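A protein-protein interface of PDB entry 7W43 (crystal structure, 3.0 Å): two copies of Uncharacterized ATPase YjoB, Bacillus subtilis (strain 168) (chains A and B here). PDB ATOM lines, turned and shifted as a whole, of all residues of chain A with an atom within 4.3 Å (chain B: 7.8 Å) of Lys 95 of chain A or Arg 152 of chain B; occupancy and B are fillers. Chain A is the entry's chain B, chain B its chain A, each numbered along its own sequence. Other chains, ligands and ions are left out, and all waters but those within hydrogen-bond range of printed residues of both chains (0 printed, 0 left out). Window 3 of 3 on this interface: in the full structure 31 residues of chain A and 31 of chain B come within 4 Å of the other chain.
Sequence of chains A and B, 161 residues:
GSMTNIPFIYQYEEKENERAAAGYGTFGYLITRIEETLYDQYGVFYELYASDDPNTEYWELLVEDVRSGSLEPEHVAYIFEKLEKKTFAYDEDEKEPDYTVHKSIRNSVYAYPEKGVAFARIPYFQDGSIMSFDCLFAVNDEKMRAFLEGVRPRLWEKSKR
No position is printed for both chains.
Tyr 58 of chain B touches Tyr 90 of chain A.
CD1 of Leu 148 of chain B touches CG of Tyr 90 of chain A (3.4 Å).
Asp 91 of chain A touches Arg 152 of chain B (O to NH2, 3.9 Å).
Arg 152 of chain B touches Glu 92 of chain A (NH2 to O, 3.8 Å).
O of Glu 94 of chain A touches NH2 of Arg 152 of chain B, at 3.6 Å.
Lys 95 of chain A touches Arg 152 of chain B.
CG of Pro 97 of chain A touches NH2 of Arg 152 of chain B (3.4 Å).
Lys 95 of chain A touches one residue of chain B.
Of chain A, only Tyr 90, Asp 91, Glu 92, Glu 94, Lys 95 and Pro 97 come within 4 Å of Arg 152 of chain B.
Printed residues of chain B within 4 Å of Pro 97 of chain A: Arg 152.
Of the printed residues of chain B, Asp 91 of chain A touches Arg 152 (3.9 Å).
Leu 61 of chain B touches none of the printed residues of chain A.
The nearest printed residue of chain A that does not touch Arg 152 of chain B is Asp 93 of chain A (5.4 Å).
The nearest printed residue of chain A that does not touch Leu 148 of chain B is Pro 97 of chain A (6.4 Å).
N of Asp 93 of chain A lies close to OD2 of Asp 91 of chain A (3.3 Å).
The backbone NH (N) of Glu 94 of chain A is in hydrogen-bond range of the side-chain carboxylate (OD1) of Asp 91 of chain A.
The side-chain carboxylate (OE2) of Glu 57 of chain B lies within hydrogen-bond range of the side-chain hydroxyl (OH) of Tyr 90 of chain A, 3.2 Å away.
OE1 of Glu 92 of chain A is in hydrogen-bond range of N of Glu 57 of chain B, 2.7 Å away.
NE of Arg 152 of chain B sits at hydrogen-bond distance from OH of Tyr 90 of chain A (2.7 Å).
Hydrophobic or aromatic side chains of chain B that line the printed part of chain A: Tyr 58 and Leu 148.
Among the printed residues, no Asp or Glu carboxylate lies within 4 Å of a Lys or Arg side-chain nitrogen of the other chain.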
ATOM      1  N   TYR A  90     -27.045 -11.607  -3.882  1.00  0.00           N
ATOM      2  CA  TYR A  90     -26.388 -11.984  -5.130  1.00  0.00           C
ATOM      3  C   TYR A  90     -27.384 -11.855  -6.274  1.00  0.00           C
ATOM      4  O   TYR A  90     -28.356 -12.615  -6.347  1.00  0.00           O
ATOM      5  CB  TYR A  90     -25.840 -13.408  -5.047  1.00  0.00           C
ATOM      6  CG  TYR A  90     -25.069 -13.848  -6.274  1.00  0.00           C
ATOM      7  CD1 TYR A  90     -23.842 -13.280  -6.585  1.00  0.00           C
ATOM      8  CD2 TYR A  90     -25.563 -14.841  -7.114  1.00  0.00           C
ATOM      9  CE1 TYR A  90     -23.130 -13.679  -7.699  1.00  0.00           C
ATOM     10  CE2 TYR A  90     -24.855 -15.249  -8.233  1.00  0.00           C
ATOM     11  CZ  TYR A  90     -23.639 -14.663  -8.519  1.00  0.00           C
ATOM     12  OH  TYR A  90     -22.924 -15.055  -9.627  1.00  0.00           O
ATOM     13  N   ASP A  91     -27.141 -10.898  -7.165  1.00  0.00           N
ATOM     14  CA  ASP A  91     -27.907 -10.750  -8.395  1.00  0.00           C
ATOM     15  C   ASP A  91     -26.973 -10.986  -9.571  1.00  0.00           C
ATOM     16  O   ASP A  91     -25.953 -10.302  -9.703  1.00  0.00           O
ATOM     17  CB  ASP A  91     -28.555  -9.368  -8.492  1.00  0.00           C
ATOM     18  CG  ASP A  91     -29.208  -9.127  -9.838  1.00  0.00           C
ATOM     19  OD1 ASP A  91     -29.045  -8.020 -10.392  1.00  0.00           O
ATOM     20  OD2 ASP A  91     -29.879 -10.050 -10.348  1.00  0.00           O
ATOM     21  N   GLU A  92     -27.324 -11.955 -10.418  1.00  0.00           N
ATOM     22  CA  GLU A  92     -26.492 -12.274 -11.573  1.00  0.00           C
ATOM     23  C   GLU A  92     -26.406 -11.105 -12.541  1.00  0.00           C
ATOM     24  O   GLU A  92     -25.366 -10.897 -13.178  1.00  0.00           O
ATOM     25  CB  GLU A  92     -27.045 -13.511 -12.275  1.00  0.00           C
ATOM     26  CG  GLU A  92     -27.432 -14.617 -11.313  1.00  0.00           C
ATOM     27  CD  GLU A  92     -28.443 -15.572 -11.906  1.00  0.00           C
ATOM     28  OE1 GLU A  92     -28.789 -16.562 -11.229  1.00  0.00           O
ATOM     29  OE2 GLU A  92     -28.899 -15.326 -13.042  1.00  0.00           O
ATOM     30  N   ASP A  93     -27.485 -10.329 -12.664  1.00  0.00           N
ATOM     31  CA  ASP A  93     -27.481  -9.197 -13.582  1.00  0.00           C
ATOM     32  C   ASP A  93     -26.579  -8.075 -13.083  1.00  0.00           C
ATOM     33  O   ASP A  93     -26.089  -7.272 -13.886  1.00  0.00           O
ATOM     34  CB  ASP A  93     -28.909  -8.698 -13.788  1.00  0.00           C
ATOM     35  CG  ASP A  93     -29.899  -9.837 -13.951  1.00  0.00           C
ATOM     36  OD1 ASP A  93     -29.512 -10.889 -14.503  1.00  0.00           O
ATOM     37  OD2 ASP A  93     -31.061  -9.685 -13.517  1.00  0.00           O
ATOM     38  N   GLU A  94     -26.352  -8.002 -11.773  1.00  0.00           N
ATOM     39  CA  GLU A  94     -25.370  -7.072 -11.233  1.00  0.00           C
ATOM     40  C   GLU A  94     -23.978  -7.452 -11.723  1.00  0.00           C
ATOM     41  O   GLU A  94     -23.540  -8.595 -11.558  1.00  0.00           O
ATOM     42  CB  GLU A  94     -25.418  -7.077  -9.703  1.00  0.00           C
ATOM     43  CG  GLU A  94     -25.062  -5.749  -9.044  1.00  0.00           C
ATOM     44  CD  GLU A  94     -26.178  -4.725  -9.132  1.00  0.00           C
ATOM     45  OE1 GLU A  94     -27.356  -5.113  -8.979  1.00  0.00           O
ATOM     46  OE2 GLU A  94     -25.879  -3.531  -9.339  1.00  0.00           O
ATOM     47  N   LYS A  95     -23.285  -6.492 -12.336  1.00  0.00           N
ATOM     48  CA  LYS A  95     -21.975  -6.790 -12.907  1.00  0.00           C
ATOM     49  C   LYS A  95     -20.945  -7.085 -11.822  1.00  0.00           C
ATOM     50  O   LYS A  95     -20.110  -7.982 -11.981  1.00  0.00           O
ATOM     51  CB  LYS A  95     -21.510  -5.638 -13.798  1.00  0.00           C
ATOM     52  CG  LYS A  95     -22.538  -5.199 -14.831  1.00  0.00           C
ATOM     53  CD  LYS A  95     -22.685  -6.235 -15.935  1.00  0.00           C
ATOM     54  CE  LYS A  95     -21.413  -6.348 -16.760  1.00  0.00           C
ATOM     55  NZ  LYS A  95     -21.019  -5.051 -17.373  1.00  0.00           N
ATOM     56  N   GLU A  96     -20.988  -6.347 -10.714  1.00  0.00           N
ATOM     57  CA  GLU A  96     -20.070  -6.586  -9.605  1.00  0.00           C
ATOM     58  C   GLU A  96     -20.840  -7.133  -8.413  1.00  0.00           C
ATOM     59  O   GLU A  96     -21.673  -6.415  -7.837  1.00  0.00           O
ATOM     60  CB  GLU A  96     -19.329  -5.305  -9.225  1.00  0.00           C
ATOM     61  CG  GLU A  96     -17.844  -5.518  -8.996  1.00  0.00           C
ATOM     62  CD  GLU A  96     -17.158  -6.165 -10.185  1.00  0.00           C
ATOM     63  OE1 GLU A  96     -16.676  -7.309 -10.046  1.00  0.00           O
ATOM     64  OE2 GLU A  96     -17.102  -5.531 -11.260  1.00  0.00           O
ATOM     65  N   PRO A  97     -20.602  -8.378  -8.006  1.00  0.00           N
ATOM     66  CA  PRO A  97     -21.451  -8.996  -6.984  1.00  0.00           C
ATOM     67  C   PRO A  97     -21.055  -8.587  -5.574  1.00  0.00           C
ATOM     68  O   PRO A  97     -19.872  -8.480  -5.239  1.00  0.00           O
ATOM     69  CB  PRO A  97     -21.220 -10.499  -7.203  1.00  0.00           C
ATOM     70  CG  PRO A  97     -20.570 -10.599  -8.570  1.00  0.00           C
ATOM     71  CD  PRO A  97     -19.726  -9.371  -8.639  1.00  0.00           C
ATOM     72  N   GLU B  57     -27.910 -19.082 -11.758  1.00  0.00           N
ATOM     73  CA  GLU B  57     -26.588 -19.466 -12.245  1.00  0.00           C
ATOM     74  C   GLU B  57     -26.016 -20.649 -11.470  1.00  0.00           C
ATOM     75  O   GLU B  57     -25.545 -21.620 -12.071  1.00  0.00           O
ATOM     76  CB  GLU B  57     -25.633 -18.273 -12.204  1.00  0.00           C
ATOM     77  CG  GLU B  57     -25.677 -17.417 -13.466  1.00  0.00           C
ATOM     78  CD  GLU B  57     -24.614 -16.336 -13.477  1.00  0.00           C
ATOM     79  OE1 GLU B  57     -24.463 -15.660 -14.518  1.00  0.00           O
ATOM     80  OE2 GLU B  57     -23.924 -16.169 -12.451  1.00  0.00           O
ATOM     81  N   TYR B  58     -26.023 -20.594 -10.136  1.00  0.00           N
ATOM     82  CA  TYR B  58     -25.501 -21.749  -9.417  1.00  0.00           C
ATOM     83  C   TYR B  58     -26.478 -22.913  -9.432  1.00  0.00           C
ATOM     84  O   TYR B  58     -26.053 -24.063  -9.275  1.00  0.00           O
ATOM     85  CB  TYR B  58     -25.130 -21.414  -7.968  1.00  0.00           C
ATOM     86  CG  TYR B  58     -26.121 -20.578  -7.191  1.00  0.00           C
ATOM     87  CD1 TYR B  58     -26.180 -19.199  -7.341  1.00  0.00           C
ATOM     88  CD2 TYR B  58     -26.990 -21.177  -6.289  1.00  0.00           C
ATOM     89  CE1 TYR B  58     -27.081 -18.443  -6.616  1.00  0.00           C
ATOM     90  CE2 TYR B  58     -27.893 -20.432  -5.570  1.00  0.00           C
ATOM     91  CZ  TYR B  58     -27.936 -19.069  -5.733  1.00  0.00           C
ATOM     92  OH  TYR B  58     -28.838 -18.329  -5.008  1.00  0.00           O
ATOM     93  N   LEU B  61     -25.502 -24.652 -12.479  1.00  0.00           N
ATOM     94  CA  LEU B  61     -24.269 -25.403 -12.254  1.00  0.00           C
ATOM     95  C   LEU B  61     -24.544 -26.753 -11.608  1.00  0.00           C
ATOM     96  O   LEU B  61     -23.842 -27.731 -11.887  1.00  0.00           O
ATOM     97  CB  LEU B  61     -23.296 -24.599 -11.396  1.00  0.00           C
ATOM     98  CG  LEU B  61     -22.402 -23.612 -12.136  1.00  0.00           C
ATOM     99  CD1 LEU B  61     -21.632 -22.767 -11.144  1.00  0.00           C
ATOM    100  CD2 LEU B  61     -21.445 -24.381 -13.033  1.00  0.00           C
ATOM    101  N   PHE B 147     -19.189 -20.284  -1.295  1.00  0.00           N
ATOM    102  CA  PHE B 147     -19.883 -20.843  -2.452  1.00  0.00           C
ATOM    103  C   PHE B 147     -20.246 -19.754  -3.453  1.00  0.00           C
ATOM    104  O   PHE B 147     -19.940 -19.868  -4.645  1.00  0.00           O
ATOM    105  CB  PHE B 147     -21.135 -21.600  -2.012  1.00  0.00           C
ATOM    106  CG  PHE B 147     -21.775 -22.398  -3.116  1.00  0.00           C
ATOM    107  CD1 PHE B 147     -22.752 -21.833  -3.919  1.00  0.00           C
ATOM    108  CD2 PHE B 147     -21.394 -23.706  -3.356  1.00  0.00           C
ATOM    109  CE1 PHE B 147     -23.339 -22.558  -4.936  1.00  0.00           C
ATOM    110  CE2 PHE B 147     -21.979 -24.436  -4.373  1.00  0.00           C
ATOM    111  CZ  PHE B 147     -22.953 -23.861  -5.163  1.00  0.00           C
ATOM    112  N   LEU B 148     -20.907 -18.691  -2.983  1.00  0.00           N
ATOM    113  CA  LEU B 148     -21.329 -17.618  -3.877  1.00  0.00           C
ATOM    114  C   LEU B 148     -20.151 -17.026  -4.636  1.00  0.00           C
ATOM    115  O   LEU B 148     -20.294 -16.631  -5.799  1.00  0.00           O
ATOM    116  CB  LEU B 148     -22.046 -16.522  -3.087  1.00  0.00           C
ATOM    117  CG  LEU B 148     -23.559 -16.629  -2.877  1.00  0.00           C
ATOM    118  CD1 LEU B 148     -24.304 -16.486  -4.195  1.00  0.00           C
ATOM    119  CD2 LEU B 148     -23.942 -17.918  -2.176  1.00  0.00           C
ATOM    120  N   GLU B 149     -18.979 -16.964  -4.001  1.00  0.00           N
ATOM    121  CA  GLU B 149     -17.796 -16.462  -4.688  1.00  0.00           C
ATOM    122  C   GLU B 149     -17.273 -17.472  -5.701  1.00  0.00           C
ATOM    123  O   GLU B 149     -16.844 -17.093  -6.796  1.00  0.00           O
ATOM    124  CB  GLU B 149     -16.711 -16.108  -3.675  1.00  0.00           C
ATOM    125  CG  GLU B 149     -16.994 -14.852  -2.875  1.00  0.00           C
ATOM    126  CD  GLU B 149     -16.269 -14.837  -1.547  1.00  0.00           C
ATOM    127  OE1 GLU B 149     -16.356 -13.816  -0.833  1.00  0.00           O
ATOM    128  OE2 GLU B 149     -15.614 -15.848  -1.216  1.00  0.00           O
ATOM    129  N   GLY B 150     -17.307 -18.759  -5.358  1.00  0.00           N
ATOM    130  CA  GLY B 150     -16.784 -19.788  -6.239  1.00  0.00           C
ATOM    131  C   GLY B 150     -17.620 -20.051  -7.475  1.00  0.00           C
ATOM    132  O   GLY B 150     -17.152 -20.763  -8.370  1.00  0.00           O
ATOM    133  N   VAL B 151     -18.829 -19.489  -7.553  1.00  0.00           N
ATOM    134  CA  VAL B 151     -19.729 -19.791  -8.667  1.00  0.00           C
ATOM    135  C   VAL B 151     -19.118 -19.347  -9.991  1.00  0.00           C
ATOM    136  O   VAL B 151     -19.099 -20.102 -10.972  1.00  0.00           O
ATOM    137  CB  VAL B 151     -21.104 -19.138  -8.440  1.00  0.00           C
ATOM    138  CG1 VAL B 151     -21.961 -19.248  -9.691  1.00  0.00           C
ATOM    139  CG2 VAL B 151     -21.807 -19.779  -7.258  1.00  0.00           C
ATOM    140  N   ARG B 152     -18.610 -18.118 -10.039  1.00  0.00           N
ATOM    141  CA  ARG B 152     -18.139 -17.546 -11.296  1.00  0.00           C
ATOM    142  C   ARG B 152     -16.803 -18.136 -11.746  1.00  0.00           C
ATOM    143  O   ARG B 152     -16.615 -18.353 -12.951  1.00  0.00           O
ATOM    144  CB  ARG B 152     -18.059 -16.022 -11.184  1.00  0.00           C
ATOM    145  CG  ARG B 152     -19.345 -15.409 -10.653  1.00  0.00           C
ATOM    146  CD  ARG B 152     -19.724 -14.147 -11.404  1.00  0.00           C
ATOM    147  NE  ARG B 152     -20.989 -13.598 -10.923  1.00  0.00           N
ATOM    148  CZ  ARG B 152     -21.494 -12.430 -11.305  1.00  0.00           C
ATOM    149  NH1 ARG B 152     -20.846 -11.678 -12.183  1.00  0.00           N
ATOM    150  NH2 ARG B 152     -22.652 -12.014 -10.810  1.00  0.00           N
ATOM    151  N   PRO B 153     -15.843 -18.398 -10.847  1.00  0.00           N
ATOM    152  CA  PRO B 153     -14.663 -19.162 -11.286  1.00  0.00           C
ATOM    153  C   PRO B 153     -15.006 -20.544 -11.816  1.00  0.00           C
ATOM    154  O   PRO B 153     -14.399 -20.996 -12.796  1.00  0.00           O
ATOM    155  CB  PRO B 153     -13.812 -19.227 -10.013  1.00  0.00           C
ATOM    156  CG  PRO B 153     -14.130 -17.961  -9.322  1.00  0.00           C
ATOM    157  CD  PRO B 153     -15.613 -17.786  -9.525  1.00  0.00           C
ATOM    158  N   ARG B 154     -15.969 -21.230 -11.192  1.00  0.00           N
ATOM    159  CA  ARG B 154     -16.432 -22.509 -11.723  1.00  0.00           C
ATOM    160  C   ARG B 154     -17.069 -22.336 -13.097  1.00  0.00           C
ATOM    161  O   ARG B 154     -16.940 -23.206 -13.967  1.00  0.00           O
ATOM    162  CB  ARG B 154     -17.425 -23.150 -10.751  1.00  0.00           C
ATOM    163  CG  ARG B 154     -16.809 -23.639  -9.447  1.00  0.00           C
ATOM    164  CD  ARG B 154     -17.492 -24.899  -8.940  1.00  0.00           C
ATOM    165  NE  ARG B 154     -18.947 -24.791  -9.009  1.00  0.00           N
ATOM    166  CZ  ARG B 154     -19.724 -24.449  -7.986  1.00  0.00           C
ATOM    167  NH1 ARG B 154     -19.190 -24.179  -6.803  1.00  0.00           N
ATOM    168  NH2 ARG B 154     -21.039 -24.376  -8.147  1.00  0.00           N
ATOM    169  N   LEU B 155     -17.762 -21.214 -13.309  1.00  0.00           N
ATOM    170  CA  LEU B 155     -18.381 -20.952 -14.605  1.00  0.00           C
ATOM    171  C   LEU B 155     -17.327 -20.675 -15.672  1.00  0.00           C
ATOM    172  O   LEU B 155     -17.458 -21.123 -16.817  1.00  0.00           O
ATOM    173  CB  LEU B 155     -19.351 -19.776 -14.478  1.00  0.00           C
ATOM    174  CG  LEU B 155     -20.740 -19.907 -15.104  1.00  0.00           C
ATOM    175  CD1 LEU B 155     -21.423 -21.161 -14.609  1.00  0.00           C
ATOM    176  CD2 LEU B 155     -21.582 -18.689 -14.768  1.00  0.00           C
ATOM    177  N   TRP B 156     -16.275 -19.939 -15.307  1.00  0.00           N
ATOM    178  CA  TRP B 156     -15.172 -19.673 -16.227  1.00  0.00           C
ATOM    179  C   TRP B 156     -14.450 -20.957 -16.621  1.00  0.00           C
ATOM    180  O   TRP B 156     -13.999 -21.098 -17.764  1.00  0.00           O
ATOM    181  CB  TRP B 156     -14.214 -18.675 -15.577  1.00  0.00           C
ATOM    182  CG  TRP B 156     -12.769 -18.808 -15.962  1.00  0.00           C
ATOM    183  CD1 TRP B 156     -11.787 -19.394 -15.220  1.00  0.00           C
ATOM    184  CD2 TRP B 156     -12.129 -18.293 -17.139  1.00  0.00           C
ATOM    185  NE1 TRP B 156     -10.584 -19.308 -15.873  1.00  0.00           N
ATOM    186  CE2 TRP B 156     -10.764 -18.634 -17.052  1.00  0.00           C
ATOM    187  CE3 TRP B 156     -12.576 -17.592 -18.260  1.00  0.00           C
ATOM    188  CZ2 TRP B 156      -9.844 -18.299 -18.043  1.00  0.00           C
ATOM    189  CZ3 TRP B 156     -11.654 -17.260 -19.243  1.00  0.00           C
ATOM    190  CH2 TRP B 156     -10.309 -17.614 -19.129  1.00  0.00           C
ATOM    191  N   GLU B 157     -14.332 -21.907 -15.689  1.00  0.00           N
ATOM    192  CA  GLU B 157     -13.712 -23.188 -16.016  1.00  0.00           C
ATOM    193  C   GLU B 157     -14.582 -23.992 -16.975  1.00  0.00           C
ATOM    194  O   GLU B 157     -14.067 -24.675 -17.867  1.00  0.00           O
ATOM    195  CB  GLU B 157     -13.444 -23.983 -14.737  1.00  0.00           C
ATOM    196  CG  GLU B 157     -12.186 -23.561 -13.999  1.00  0.00           C
ATOM    197  CD  GLU B 157     -11.408 -24.742 -13.461  1.00  0.00           C
ATOM    198  OE1 GLU B 157     -10.263 -24.543 -13.003  1.00  0.00           O
ATOM    199  OE2 GLU B 157     -11.940 -25.871 -13.501  1.00  0.00           O
ATOM    200  N   LYS B 158     -15.905 -23.925 -16.801  1.00  0.00           N
ATOM    201  CA  LYS B 158     -16.813 -24.575 -17.738  1.00  0.00           C
ATOM    202  C   LYS B 158     -16.679 -23.987 -19.138  1.00  0.00           C
ATOM    203  O   LYS B 158     -16.869 -24.698 -20.134  1.00  0.00           O
ATOM    204  CB  LYS B 158     -18.252 -24.450 -17.227  1.00  0.00           C
ATOM    205  CG  LYS B 158     -19.311 -24.298 -18.308  1.00  0.00           C
ATOM    206  CD  LYS B 158     -20.656 -23.907 -17.715  1.00  0.00           C
ATOM    207  CE  LYS B 158     -21.672 -23.605 -18.806  1.00  0.00           C
ATOM    208  NZ  LYS B 158     -23.002 -23.232 -18.247  1.00  0.00           N
ATOM    209  N   SER B 159     -16.330 -22.703 -19.235  1.00  0.00           N
ATOM    210  CA  SER B 159     -16.191 -22.065 -20.541  1.00  0.00           C
ATOM    211  C   SER B 159     -15.014 -22.639 -21.322  1.00  0.00           C
ATOM    212  O   SER B 159     -15.100 -22.811 -22.543  1.00  0.00           O
ATOM    213  CB  SER B 159     -16.036 -20.554 -20.369  1.00  0.00           C
ATOM    214  OG  SER B 159     -17.049 -20.031 -19.528  1.00  0.00           O
